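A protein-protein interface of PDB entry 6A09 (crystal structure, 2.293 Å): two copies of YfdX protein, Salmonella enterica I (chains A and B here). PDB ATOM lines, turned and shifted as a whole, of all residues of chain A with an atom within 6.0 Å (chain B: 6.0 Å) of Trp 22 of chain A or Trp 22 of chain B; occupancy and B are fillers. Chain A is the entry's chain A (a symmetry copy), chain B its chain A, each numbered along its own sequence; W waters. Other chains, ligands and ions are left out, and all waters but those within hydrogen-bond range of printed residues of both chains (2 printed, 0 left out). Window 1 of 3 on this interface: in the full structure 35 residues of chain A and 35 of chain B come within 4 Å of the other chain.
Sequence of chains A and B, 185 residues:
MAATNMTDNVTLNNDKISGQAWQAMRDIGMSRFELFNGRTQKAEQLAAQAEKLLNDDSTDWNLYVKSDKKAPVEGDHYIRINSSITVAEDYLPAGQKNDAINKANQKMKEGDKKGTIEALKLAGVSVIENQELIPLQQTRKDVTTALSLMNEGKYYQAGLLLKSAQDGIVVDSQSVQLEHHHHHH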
ATOM      1  N   MET A   6     -31.720 -10.921 -23.504  1.00  0.00           N
ATOM      2  CA  MET A   6     -31.764 -12.306 -23.029  1.00  0.00           C
ATOM      3  C   MET A   6     -32.963 -13.121 -23.566  1.00  0.00           C
ATOM      4  O   MET A   6     -32.923 -14.356 -23.551  1.00  0.00           O
ATOM      5  CB  MET A   6     -31.761 -12.345 -21.497  1.00  0.00           C
ATOM      6  CG  MET A   6     -31.303 -13.683 -20.920  1.00  0.00           C
ATOM      7  SD  MET A   6     -31.883 -13.903 -19.213  1.00  0.00           S
ATOM      8  CE  MET A   6     -33.669 -13.791 -19.423  1.00  0.00           C
ATOM      9  N   SER A  18     -30.292 -16.948 -29.968  1.00  0.00           N
ATOM     10  CA  SER A  18     -30.184 -17.127 -28.526  1.00  0.00           C
ATOM     11  C   SER A  18     -29.910 -15.786 -27.854  1.00  0.00           C
ATOM     12  O   SER A  18     -28.831 -15.199 -28.023  1.00  0.00           O
ATOM     13  CB  SER A  18     -29.090 -18.131 -28.190  1.00  0.00           C
ATOM     14  OG  SER A  18     -28.845 -18.138 -26.787  1.00  0.00           O
ATOM     15  N   GLY A  19     -30.885 -15.313 -27.069  1.00  0.00           N
ATOM     16  CA  GLY A  19     -30.678 -14.130 -26.259  1.00  0.00           C
ATOM     17  C   GLY A  19     -29.891 -14.423 -25.005  1.00  0.00           C
ATOM     18  O   GLY A  19     -29.171 -13.554 -24.503  1.00  0.00           O
ATOM     19  N   GLN A  20     -29.988 -15.648 -24.495  1.00  0.00           N
ATOM     20  CA  GLN A  20     -29.106 -16.051 -23.407  1.00  0.00           C
ATOM     21  C   GLN A  20     -27.639 -15.995 -23.824  1.00  0.00           C
ATOM     22  O   GLN A  20     -26.798 -15.456 -23.094  1.00  0.00           O
ATOM     23  CB  GLN A  20     -29.462 -17.450 -22.942  1.00  0.00           C
ATOM     24  CG  GLN A  20     -30.779 -17.543 -22.230  1.00  0.00           C
ATOM     25  CD  GLN A  20     -31.023 -18.954 -21.790  1.00  0.00           C
ATOM     26  OE1 GLN A  20     -31.148 -19.856 -22.621  1.00  0.00           O
ATOM     27  NE2 GLN A  20     -31.026 -19.177 -20.487  1.00  0.00           N
ATOM     28  N   ALA A  21     -27.303 -16.579 -24.980  1.00  0.00           N
ATOM     29  CA  ALA A  21     -25.911 -16.538 -25.411  1.00  0.00           C
ATOM     30  C   ALA A  21     -25.471 -15.101 -25.669  1.00  0.00           C
ATOM     31  O   ALA A  21     -24.347 -14.710 -25.322  1.00  0.00           O
ATOM     32  CB  ALA A  21     -25.712 -17.400 -26.651  1.00  0.00           C
ATOM     33  N   TRP A  22     -26.348 -14.289 -26.254  1.00  0.00           N
ATOM     34  CA  TRP A  22     -26.003 -12.881 -26.429  1.00  0.00           C
ATOM     35  C   TRP A  22     -25.652 -12.226 -25.089  1.00  0.00           C
ATOM     36  O   TRP A  22     -24.674 -11.481 -24.988  1.00  0.00           O
ATOM     37  CB  TRP A  22     -27.144 -12.133 -27.126  1.00  0.00           C
ATOM     38  CG  TRP A  22     -26.707 -10.763 -27.466  1.00  0.00           C
ATOM     39  CD1 TRP A  22     -26.090 -10.352 -28.628  1.00  0.00           C
ATOM     40  CD2 TRP A  22     -26.766  -9.623 -26.617  1.00  0.00           C
ATOM     41  NE1 TRP A  22     -25.786  -9.022 -28.549  1.00  0.00           N
ATOM     42  CE2 TRP A  22     -26.188  -8.546 -27.327  1.00  0.00           C
ATOM     43  CE3 TRP A  22     -27.251  -9.404 -25.318  1.00  0.00           C
ATOM     44  CZ2 TRP A  22     -26.093  -7.265 -26.790  1.00  0.00           C
ATOM     45  CZ3 TRP A  22     -27.150  -8.133 -24.782  1.00  0.00           C
ATOM     46  CH2 TRP A  22     -26.576  -7.077 -25.520  1.00  0.00           C
ATOM     47  N   GLN A  23     -26.419 -12.520 -24.039  1.00  0.00           N
ATOM     48  CA  GLN A  23     -26.198 -11.869 -22.754  1.00  0.00           C
ATOM     49  C   GLN A  23     -24.913 -12.359 -22.098  1.00  0.00           C
ATOM     50  O   GLN A  23     -24.224 -11.584 -21.419  1.00  0.00           O
ATOM     51  CB  GLN A  23     -27.400 -12.111 -21.828  1.00  0.00           C
ATOM     52  CG  GLN A  23     -27.280 -11.458 -20.436  1.00  0.00           C
ATOM     53  CD  GLN A  23     -27.123  -9.945 -20.531  1.00  0.00           C
ATOM     54  OE1 GLN A  23     -27.894  -9.280 -21.216  1.00  0.00           O
ATOM     55  NE2 GLN A  23     -26.105  -9.403 -19.871  1.00  0.00           N
ATOM     56  N   ALA A  24     -24.591 -13.646 -22.276  1.00  0.00           N
ATOM     57  CA  ALA A  24     -23.329 -14.199 -21.780  1.00  0.00           C
ATOM     58  C   ALA A  24     -22.127 -13.490 -22.399  1.00  0.00           C
ATOM     59  O   ALA A  24     -21.184 -13.123 -21.687  1.00  0.00           O
ATOM     60  CB  ALA A  24     -23.266 -15.707 -22.061  1.00  0.00           C
ATOM     61  N   MET A  25     -22.144 -13.281 -23.724  1.00  0.00           N
ATOM     62  CA  MET A  25     -21.031 -12.573 -24.364  1.00  0.00           C
ATOM     63  C   MET A  25     -20.902 -11.167 -23.818  1.00  0.00           C
ATOM     64  O   MET A  25     -19.790 -10.688 -23.575  1.00  0.00           O
ATOM     65  CB  MET A  25     -21.193 -12.530 -25.882  1.00  0.00           C
ATOM     66  CG  MET A  25     -21.296 -13.922 -26.504  1.00  0.00           C
ATOM     67  SD  MET A  25     -20.068 -15.115 -25.899  1.00  0.00           S
ATOM     68  CE  MET A  25     -18.514 -14.315 -26.330  1.00  0.00           C
ATOM     69  N   ARG A  26     -22.036 -10.501 -23.581  1.00  0.00           N
ATOM     70  CA  ARG A  26     -21.999  -9.194 -22.937  1.00  0.00           C
ATOM     71  C   ARG A  26     -21.388  -9.294 -21.538  1.00  0.00           C
ATOM     72  O   ARG A  26     -20.518  -8.497 -21.177  1.00  0.00           O
ATOM     73  CB  ARG A  26     -23.410  -8.601 -22.896  1.00  0.00           C
ATOM     74  CG  ARG A  26     -23.554  -7.369 -22.012  1.00  0.00           C
ATOM     75  CD  ARG A  26     -22.750  -6.200 -22.517  1.00  0.00           C
ATOM     76  NE  ARG A  26     -23.078  -4.970 -21.799  1.00  0.00           N
ATOM     77  CZ  ARG A  26     -22.259  -3.923 -21.715  1.00  0.00           C
ATOM     78  NH1 ARG A  26     -21.064  -3.973 -22.283  1.00  0.00           N
ATOM     79  NH2 ARG A  26     -22.615  -2.828 -21.052  1.00  0.00           N
ATOM     80  N   ASP A  27     -21.793 -10.300 -20.754  1.00  0.00           N
ATOM     81  CA  ASP A  27     -21.230 -10.474 -19.414  1.00  0.00           C
ATOM     82  C   ASP A  27     -19.739 -10.796 -19.467  1.00  0.00           C
ATOM     83  O   ASP A  27     -18.969 -10.357 -18.603  1.00  0.00           O
ATOM     84  CB  ASP A  27     -21.951 -11.593 -18.659  1.00  0.00           C
ATOM     85  CG  ASP A  27     -23.397 -11.272 -18.344  1.00  0.00           C
ATOM     86  OD1 ASP A  27     -23.786 -10.087 -18.419  1.00  0.00           O
ATOM     87  OD2 ASP A  27     -24.138 -12.230 -18.003  1.00  0.00           O
ATOM     88  N   ILE A  81     -26.281 -15.594 -32.092  1.00  0.00           N
ATOM     89  CA  ILE A  81     -26.510 -14.718 -30.947  1.00  0.00           C
ATOM     90  C   ILE A  81     -26.997 -13.324 -31.338  1.00  0.00           C
ATOM     91  O   ILE A  81     -27.418 -12.562 -30.453  1.00  0.00           O
ATOM     92  CB  ILE A  81     -25.260 -14.612 -30.041  1.00  0.00           C
ATOM     93  CG1 ILE A  81     -24.155 -13.738 -30.667  1.00  0.00           C
ATOM     94  CG2 ILE A  81     -24.732 -15.995 -29.689  1.00  0.00           C
ATOM     95  CD1 ILE A  81     -22.996 -13.451 -29.693  1.00  0.00           C
ATOM     96  N   ASN A  82     -26.956 -12.953 -32.615  1.00  0.00           N
ATOM     97  CA  ASN A  82     -27.447 -11.648 -33.025  1.00  0.00           C
ATOM     98  C   ASN A  82     -27.605 -11.645 -34.533  1.00  0.00           C
ATOM     99  O   ASN A  82     -26.894 -12.356 -35.245  1.00  0.00           O
ATOM    100  CB  ASN A  82     -26.514 -10.503 -32.603  1.00  0.00           C
ATOM    101  CG  ASN A  82     -27.172  -9.114 -32.760  1.00  0.00           C
ATOM    102  OD1 ASN A  82     -28.040  -8.738 -31.987  1.00  0.00           O
ATOM    103  ND2 ASN A  82     -26.773  -8.378 -33.787  1.00  0.00           N
ATOM    104  N   GLU A 132     -24.261 -12.854 -36.189  1.00  0.00           N
ATOM    105  CA  GLU A 132     -23.194 -13.056 -35.235  1.00  0.00           C
ATOM    106  C   GLU A 132     -23.329 -14.443 -34.596  1.00  0.00           C
ATOM    107  O   GLU A 132     -24.416 -14.833 -34.137  1.00  0.00           O
ATOM    108  CB  GLU A 132     -23.260 -11.946 -34.194  1.00  0.00           C
ATOM    109  CG  GLU A 132     -22.112 -11.880 -33.248  1.00  0.00           C
ATOM    110  CD  GLU A 132     -22.176 -10.653 -32.343  1.00  0.00           C
ATOM    111  OE1 GLU A 132     -23.282 -10.088 -32.175  1.00  0.00           O
ATOM    112  OE2 GLU A 132     -21.120 -10.248 -31.798  1.00  0.00           O
ATOM    113  N   MET B   6     -28.082  -1.708 -18.351  1.00  0.00           N
ATOM    114  CA  MET B   6     -28.785  -0.455 -18.062  1.00  0.00           C
ATOM    115  C   MET B   6     -28.351   0.225 -16.743  1.00  0.00           C
ATOM    116  O   MET B   6     -28.578   1.427 -16.567  1.00  0.00           O
ATOM    117  CB  MET B   6     -30.300  -0.684 -18.047  1.00  0.00           C
ATOM    118  CG  MET B   6     -31.114   0.591 -18.259  1.00  0.00           C
ATOM    119  SD  MET B   6     -32.810   0.406 -17.638  1.00  0.00           S
ATOM    120  CE  MET B   6     -32.517   0.029 -15.900  1.00  0.00           C
ATOM    121  N   SER B  18     -22.801   5.510 -18.752  1.00  0.00           N
ATOM    122  CA  SER B  18     -24.256   5.450 -18.817  1.00  0.00           C
ATOM    123  C   SER B  18     -24.699   4.079 -19.315  1.00  0.00           C
ATOM    124  O   SER B  18     -24.473   3.725 -20.482  1.00  0.00           O
ATOM    125  CB  SER B  18     -24.800   6.552 -19.715  1.00  0.00           C
ATOM    126  OG  SER B  18     -26.191   6.356 -19.945  1.00  0.00           O
ATOM    127  N   GLY B  19     -25.354   3.318 -18.432  1.00  0.00           N
ATOM    128  CA  GLY B  19     -25.957   2.064 -18.836  1.00  0.00           C
ATOM    129  C   GLY B  19     -27.272   2.263 -19.551  1.00  0.00           C
ATOM    130  O   GLY B  19     -27.645   1.455 -20.408  1.00  0.00           O
ATOM    131  N   GLN B  20     -27.979   3.345 -19.238  1.00  0.00           N
ATOM    132  CA  GLN B  20     -29.153   3.697 -20.028  1.00  0.00           C
ATOM    133  C   GLN B  20     -28.788   3.966 -21.485  1.00  0.00           C
ATOM    134  O   GLN B  20     -29.446   3.459 -22.401  1.00  0.00           O
ATOM    135  CB  GLN B  20     -29.836   4.912 -19.429  1.00  0.00           C
ATOM    136  CG  GLN B  20     -30.504   4.652 -18.111  1.00  0.00           C
ATOM    137  CD  GLN B  20     -31.168   5.902 -17.621  1.00  0.00           C
ATOM    138  OE1 GLN B  20     -30.500   6.900 -17.346  1.00  0.00           O
ATOM    139  NE2 GLN B  20     -32.489   5.890 -17.569  1.00  0.00           N
ATOM    140  N   ALA B  21     -27.763   4.792 -21.723  1.00  0.00           N
ATOM    141  CA  ALA B  21     -27.384   5.065 -23.103  1.00  0.00           C
ATOM    142  C   ALA B  21     -26.900   3.792 -23.790  1.00  0.00           C
ATOM    143  O   ALA B  21     -27.218   3.544 -24.962  1.00  0.00           O
ATOM    144  CB  ALA B  21     -26.318   6.151 -23.158  1.00  0.00           C
ATOM    145  N   TRP B  22     -26.154   2.957 -23.072  1.00  0.00           N
ATOM    146  CA  TRP B  22     -25.753   1.681 -23.659  1.00  0.00           C
ATOM    147  C   TRP B  22     -26.975   0.872 -24.109  1.00  0.00           C
ATOM    148  O   TRP B  22     -26.983   0.298 -25.202  1.00  0.00           O
ATOM    149  CB  TRP B  22     -24.897   0.883 -22.671  1.00  0.00           C
ATOM    150  CG  TRP B  22     -24.344  -0.311 -23.344  1.00  0.00           C
ATOM    151  CD1 TRP B  22     -23.153  -0.402 -24.032  1.00  0.00           C
ATOM    152  CD2 TRP B  22     -24.983  -1.576 -23.479  1.00  0.00           C
ATOM    153  NE1 TRP B  22     -23.015  -1.653 -24.564  1.00  0.00           N
ATOM    154  CE2 TRP B  22     -24.121  -2.398 -24.241  1.00  0.00           C
ATOM    155  CE3 TRP B  22     -26.206  -2.098 -23.030  1.00  0.00           C
ATOM    156  CZ2 TRP B  22     -24.435  -3.718 -24.555  1.00  0.00           C
ATOM    157  CZ3 TRP B  22     -26.521  -3.407 -23.347  1.00  0.00           C
ATOM    158  CH2 TRP B  22     -25.635  -4.204 -24.102  1.00  0.00           C
ATOM    159  N   GLN B  23     -28.029   0.842 -23.295  1.00  0.00           N
ATOM    160  CA  GLN B  23     -29.192   0.024 -23.616  1.00  0.00           C
ATOM    161  C   GLN B  23     -29.970   0.604 -24.792  1.00  0.00           C
ATOM    162  O   GLN B  23     -30.532  -0.148 -25.600  1.00  0.00           O
ATOM    163  CB  GLN B  23     -30.099  -0.108 -22.384  1.00  0.00           C
ATOM    164  CG  GLN B  23     -31.363  -0.965 -22.606  1.00  0.00           C
ATOM    165  CD  GLN B  23     -31.017  -2.388 -23.026  1.00  0.00           C
ATOM    166  OE1 GLN B  23     -30.200  -3.044 -22.388  1.00  0.00           O
ATOM    167  NE2 GLN B  23     -31.613  -2.856 -24.118  1.00  0.00           N
ATOM    168  N   ALA B  24     -30.027   1.938 -24.885  1.00  0.00           N
ATOM    169  CA  ALA B  24     -30.657   2.603 -26.027  1.00  0.00           C
ATOM    170  C   ALA B  24     -29.972   2.229 -27.338  1.00  0.00           C
ATOM    171  O   ALA B  24     -30.646   1.910 -28.326  1.00  0.00           O
ATOM    172  CB  ALA B  24     -30.640   4.125 -25.828  1.00  0.00           C
ATOM    173  N   MET B  25     -28.631   2.255 -27.369  1.00  0.00           N
ATOM    174  CA  MET B  25     -27.922   1.870 -28.593  1.00  0.00           C
ATOM    175  C   MET B  25     -28.224   0.433 -28.961  1.00  0.00           C
ATOM    176  O   MET B  25     -28.424   0.117 -30.139  1.00  0.00           O
ATOM    177  CB  MET B  25     -26.414   2.066 -28.452  1.00  0.00           C
ATOM    178  CG  MET B  25     -26.035   3.507 -28.112  1.00  0.00           C
ATOM    179  SD  MET B  25     -26.881   4.769 -29.109  1.00  0.00           S
ATOM    180  CE  MET B  25     -26.379   4.333 -30.781  1.00  0.00           C
ATOM    181  N   ARG B  26     -28.301  -0.447 -27.960  1.00  0.00           N
ATOM    182  CA  ARG B  26     -28.713  -1.821 -28.220  1.00  0.00           C
ATOM    183  C   ARG B  26     -30.131  -1.864 -28.793  1.00  0.00           C
ATOM    184  O   ARG B  26     -30.383  -2.552 -29.787  1.00  0.00           O
ATOM    185  CB  ARG B  26     -28.599  -2.644 -26.933  1.00  0.00           C
ATOM    186  CG  ARG B  26     -29.253  -4.018 -27.001  1.00  0.00           C
ATOM    187  CD  ARG B  26     -28.587  -4.926 -28.001  1.00  0.00           C
ATOM    188  NE  ARG B  26     -29.072  -6.300 -27.887  1.00  0.00           N
ATOM    189  CZ  ARG B  26     -29.007  -7.190 -28.876  1.00  0.00           C
ATOM    190  NH1 ARG B  26     -28.501  -6.838 -30.048  1.00  0.00           N
ATOM    191  NH2 ARG B  26     -29.459  -8.428 -28.711  1.00  0.00           N
ATOM    192  N   ASP B  27     -31.059  -1.095 -28.213  1.00  0.00           N
ATOM    193  CA  ASP B  27     -32.430  -1.064 -28.727  1.00  0.00           C
ATOM    194  C   ASP B  27     -32.488  -0.488 -30.139  1.00  0.00           C
ATOM    195  O   ASP B  27     -33.294  -0.933 -30.967  1.00  0.00           O
ATOM    196  CB  ASP B  27     -33.336  -0.234 -27.816  1.00  0.00           C
ATOM    197  CG  ASP B  27     -33.538  -0.847 -26.445  1.00  0.00           C
ATOM    198  OD1 ASP B  27     -33.246  -2.050 -26.270  1.00  0.00           O
ATOM    199  OD2 ASP B  27     -34.009  -0.105 -25.547  1.00  0.00           O
ATOM    200  N   ILE B  81     -20.630   5.254 -22.954  1.00  0.00           N
ATOM    201  CA  ILE B  81     -21.600   4.165 -22.873  1.00  0.00           C
ATOM    202  C   ILE B  81     -20.959   2.798 -22.640  1.00  0.00           C
ATOM    203  O   ILE B  81     -21.684   1.833 -22.352  1.00  0.00           O
ATOM    204  CB  ILE B  81     -22.521   4.118 -24.115  1.00  0.00           C
ATOM    205  CG1 ILE B  81     -21.797   3.567 -25.360  1.00  0.00           C
ATOM    206  CG2 ILE B  81     -23.124   5.487 -24.391  1.00  0.00           C
ATOM    207  CD1 ILE B  81     -22.751   3.318 -26.545  1.00  0.00           C
ATOM    208  N   ASN B  82     -19.639   2.669 -22.755  1.00  0.00           N
ATOM    209  CA  ASN B  82     -18.994   1.391 -22.503  1.00  0.00           C
ATOM    210  C   ASN B  82     -17.503   1.625 -22.359  1.00  0.00           C
ATOM    211  O   ASN B  82     -16.950   2.561 -22.939  1.00  0.00           O
ATOM    212  CB  ASN B  82     -19.249   0.366 -23.618  1.00  0.00           C
ATOM    213  CG  ASN B  82     -18.832  -1.065 -23.214  1.00  0.00           C
ATOM    214  OD1 ASN B  82     -19.497  -1.713 -22.419  1.00  0.00           O
ATOM    215  ND2 ASN B  82     -17.711  -1.531 -23.743  1.00  0.00           N
ATOM    216  N   GLU B 132     -16.204   3.657 -25.452  1.00  0.00           N
ATOM    217  CA  GLU B 132     -17.219   3.869 -26.460  1.00  0.00           C
ATOM    218  C   GLU B 132     -18.080   5.079 -26.080  1.00  0.00           C
ATOM    219  O   GLU B 132     -18.557   5.192 -24.939  1.00  0.00           O
ATOM    220  CB  GLU B 132     -18.052   2.599 -26.582  1.00  0.00           C
ATOM    221  CG  GLU B 132     -19.015   2.566 -27.716  1.00  0.00           C
ATOM    222  CD  GLU B 132     -19.695   1.207 -27.861  1.00  0.00           C
ATOM    223  OE1 GLU B 132     -19.721   0.441 -26.869  1.00  0.00           O
ATOM    224  OE2 GLU B 132     -20.202   0.900 -28.967  1.00  0.00           O
HETATM  225  O   HOH W   1     -29.671 -10.924 -30.017  1.00  0.00           O
HETATM  226  O   HOH W   2     -21.747  -0.216 -20.417  1.00  0.00           O
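Hydrophobic or aromatic side chains of chain A that line the printed part of chain B: Trp 22.
Hydrophobic or aromatic side chains of chain B within 4 Å of the printed part of chain A: Trp 22.
Along chain B the printed residues that touch a printed residue of chain A span positions 22 to 82.
Among the printed residues, no Asp or Glu carboxylate lies within 4 Å of a Lys or Arg side-chain nitrogen of the other chain.
The backbone NH of Glu 132 of chain B lies within hydrogen-bond range of the backbone carbonyl oxygen of Asn 82 of chain B, 2.8 Å away.
O of Asn 82 of chain A lies within hydrogen-bond range of N of Glu 132 of chain A (2.8 Å).
Water W1 lies within hydrogen-bond range of O of Ile 81 of chain A (2.8 Å), NH2 of Arg 26 of chain B (2.8 Å) and OD1 of Asn 82 of chain A (3.4 Å).
Water W2 lies within hydrogen-bond range of the backbone carbonyl oxygen of Ile 81 of chain B (2.8 Å), the guanidinium group of Arg 26 of chain A (2.8 Å) and the side-chain amide oxygen of Asn 82 of chain B (3.4 Å).
Trp 22 of chain A touches its own counterpart, Trp 22 of chain B.
Trp 22 of chain A touches Arg 26 of chain B, and with the chains exchanged Arg 26 of chain A touches Trp 22 of chain B.
Arg 26 of chain A touches Asn 82 of chain B, and with the chains exchanged Asn 82 of chain A touches Arg 26 of chain B.
Positions printed for both chains: 6, 18, 19, 20, 21, 22, 23, 24, 25, 26, 27, 81, 82 and 132.
Of the 5 pairs that touch across the chains among the printed residues, 5 have their exchanged pair printed and touching as well.
CH2 of Trp 22 of chain B touches CH2 of Trp 22 of chain A (3.3 Å).
Trp 22 of chain A touches Arg 26 of chain B.
CZ2 of Trp 22 of chain B touches NE of Arg 26 of chain A (3.3 Å).
Ile 81 of chain A touches none of the printed residues of chain B.
Printed residues of chain B within 4 Å of Asn 82 of chain A: Arg 26.
Trp 22 of chain B touches just these residues of chain A: Trp 22 and Arg 26.
Of the printed residues of chain A, Arg 26 of chain B touches Trp 22 (3.3 Å) and Asn 82 (2.8 Å).
The nearest printed residue of chain B that does not touch Trp 22 of chain A is Gln 23 of chain B (6.3 Å).
The nearest printed residue of chain A that does not touch Arg 26 of chain B is Ile 81 of chain A (4.9 Å).
NH1 of Arg 26 of chain B lies within hydrogen-bond range of OD1 of Asn 82 of chain A, at 2.8 Å.
The side-chain amide oxygen (OD1) of Asn 82 of chain B is in hydrogen-bond range of the guanidinium group (NH1) of Arg 26 of chain A.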
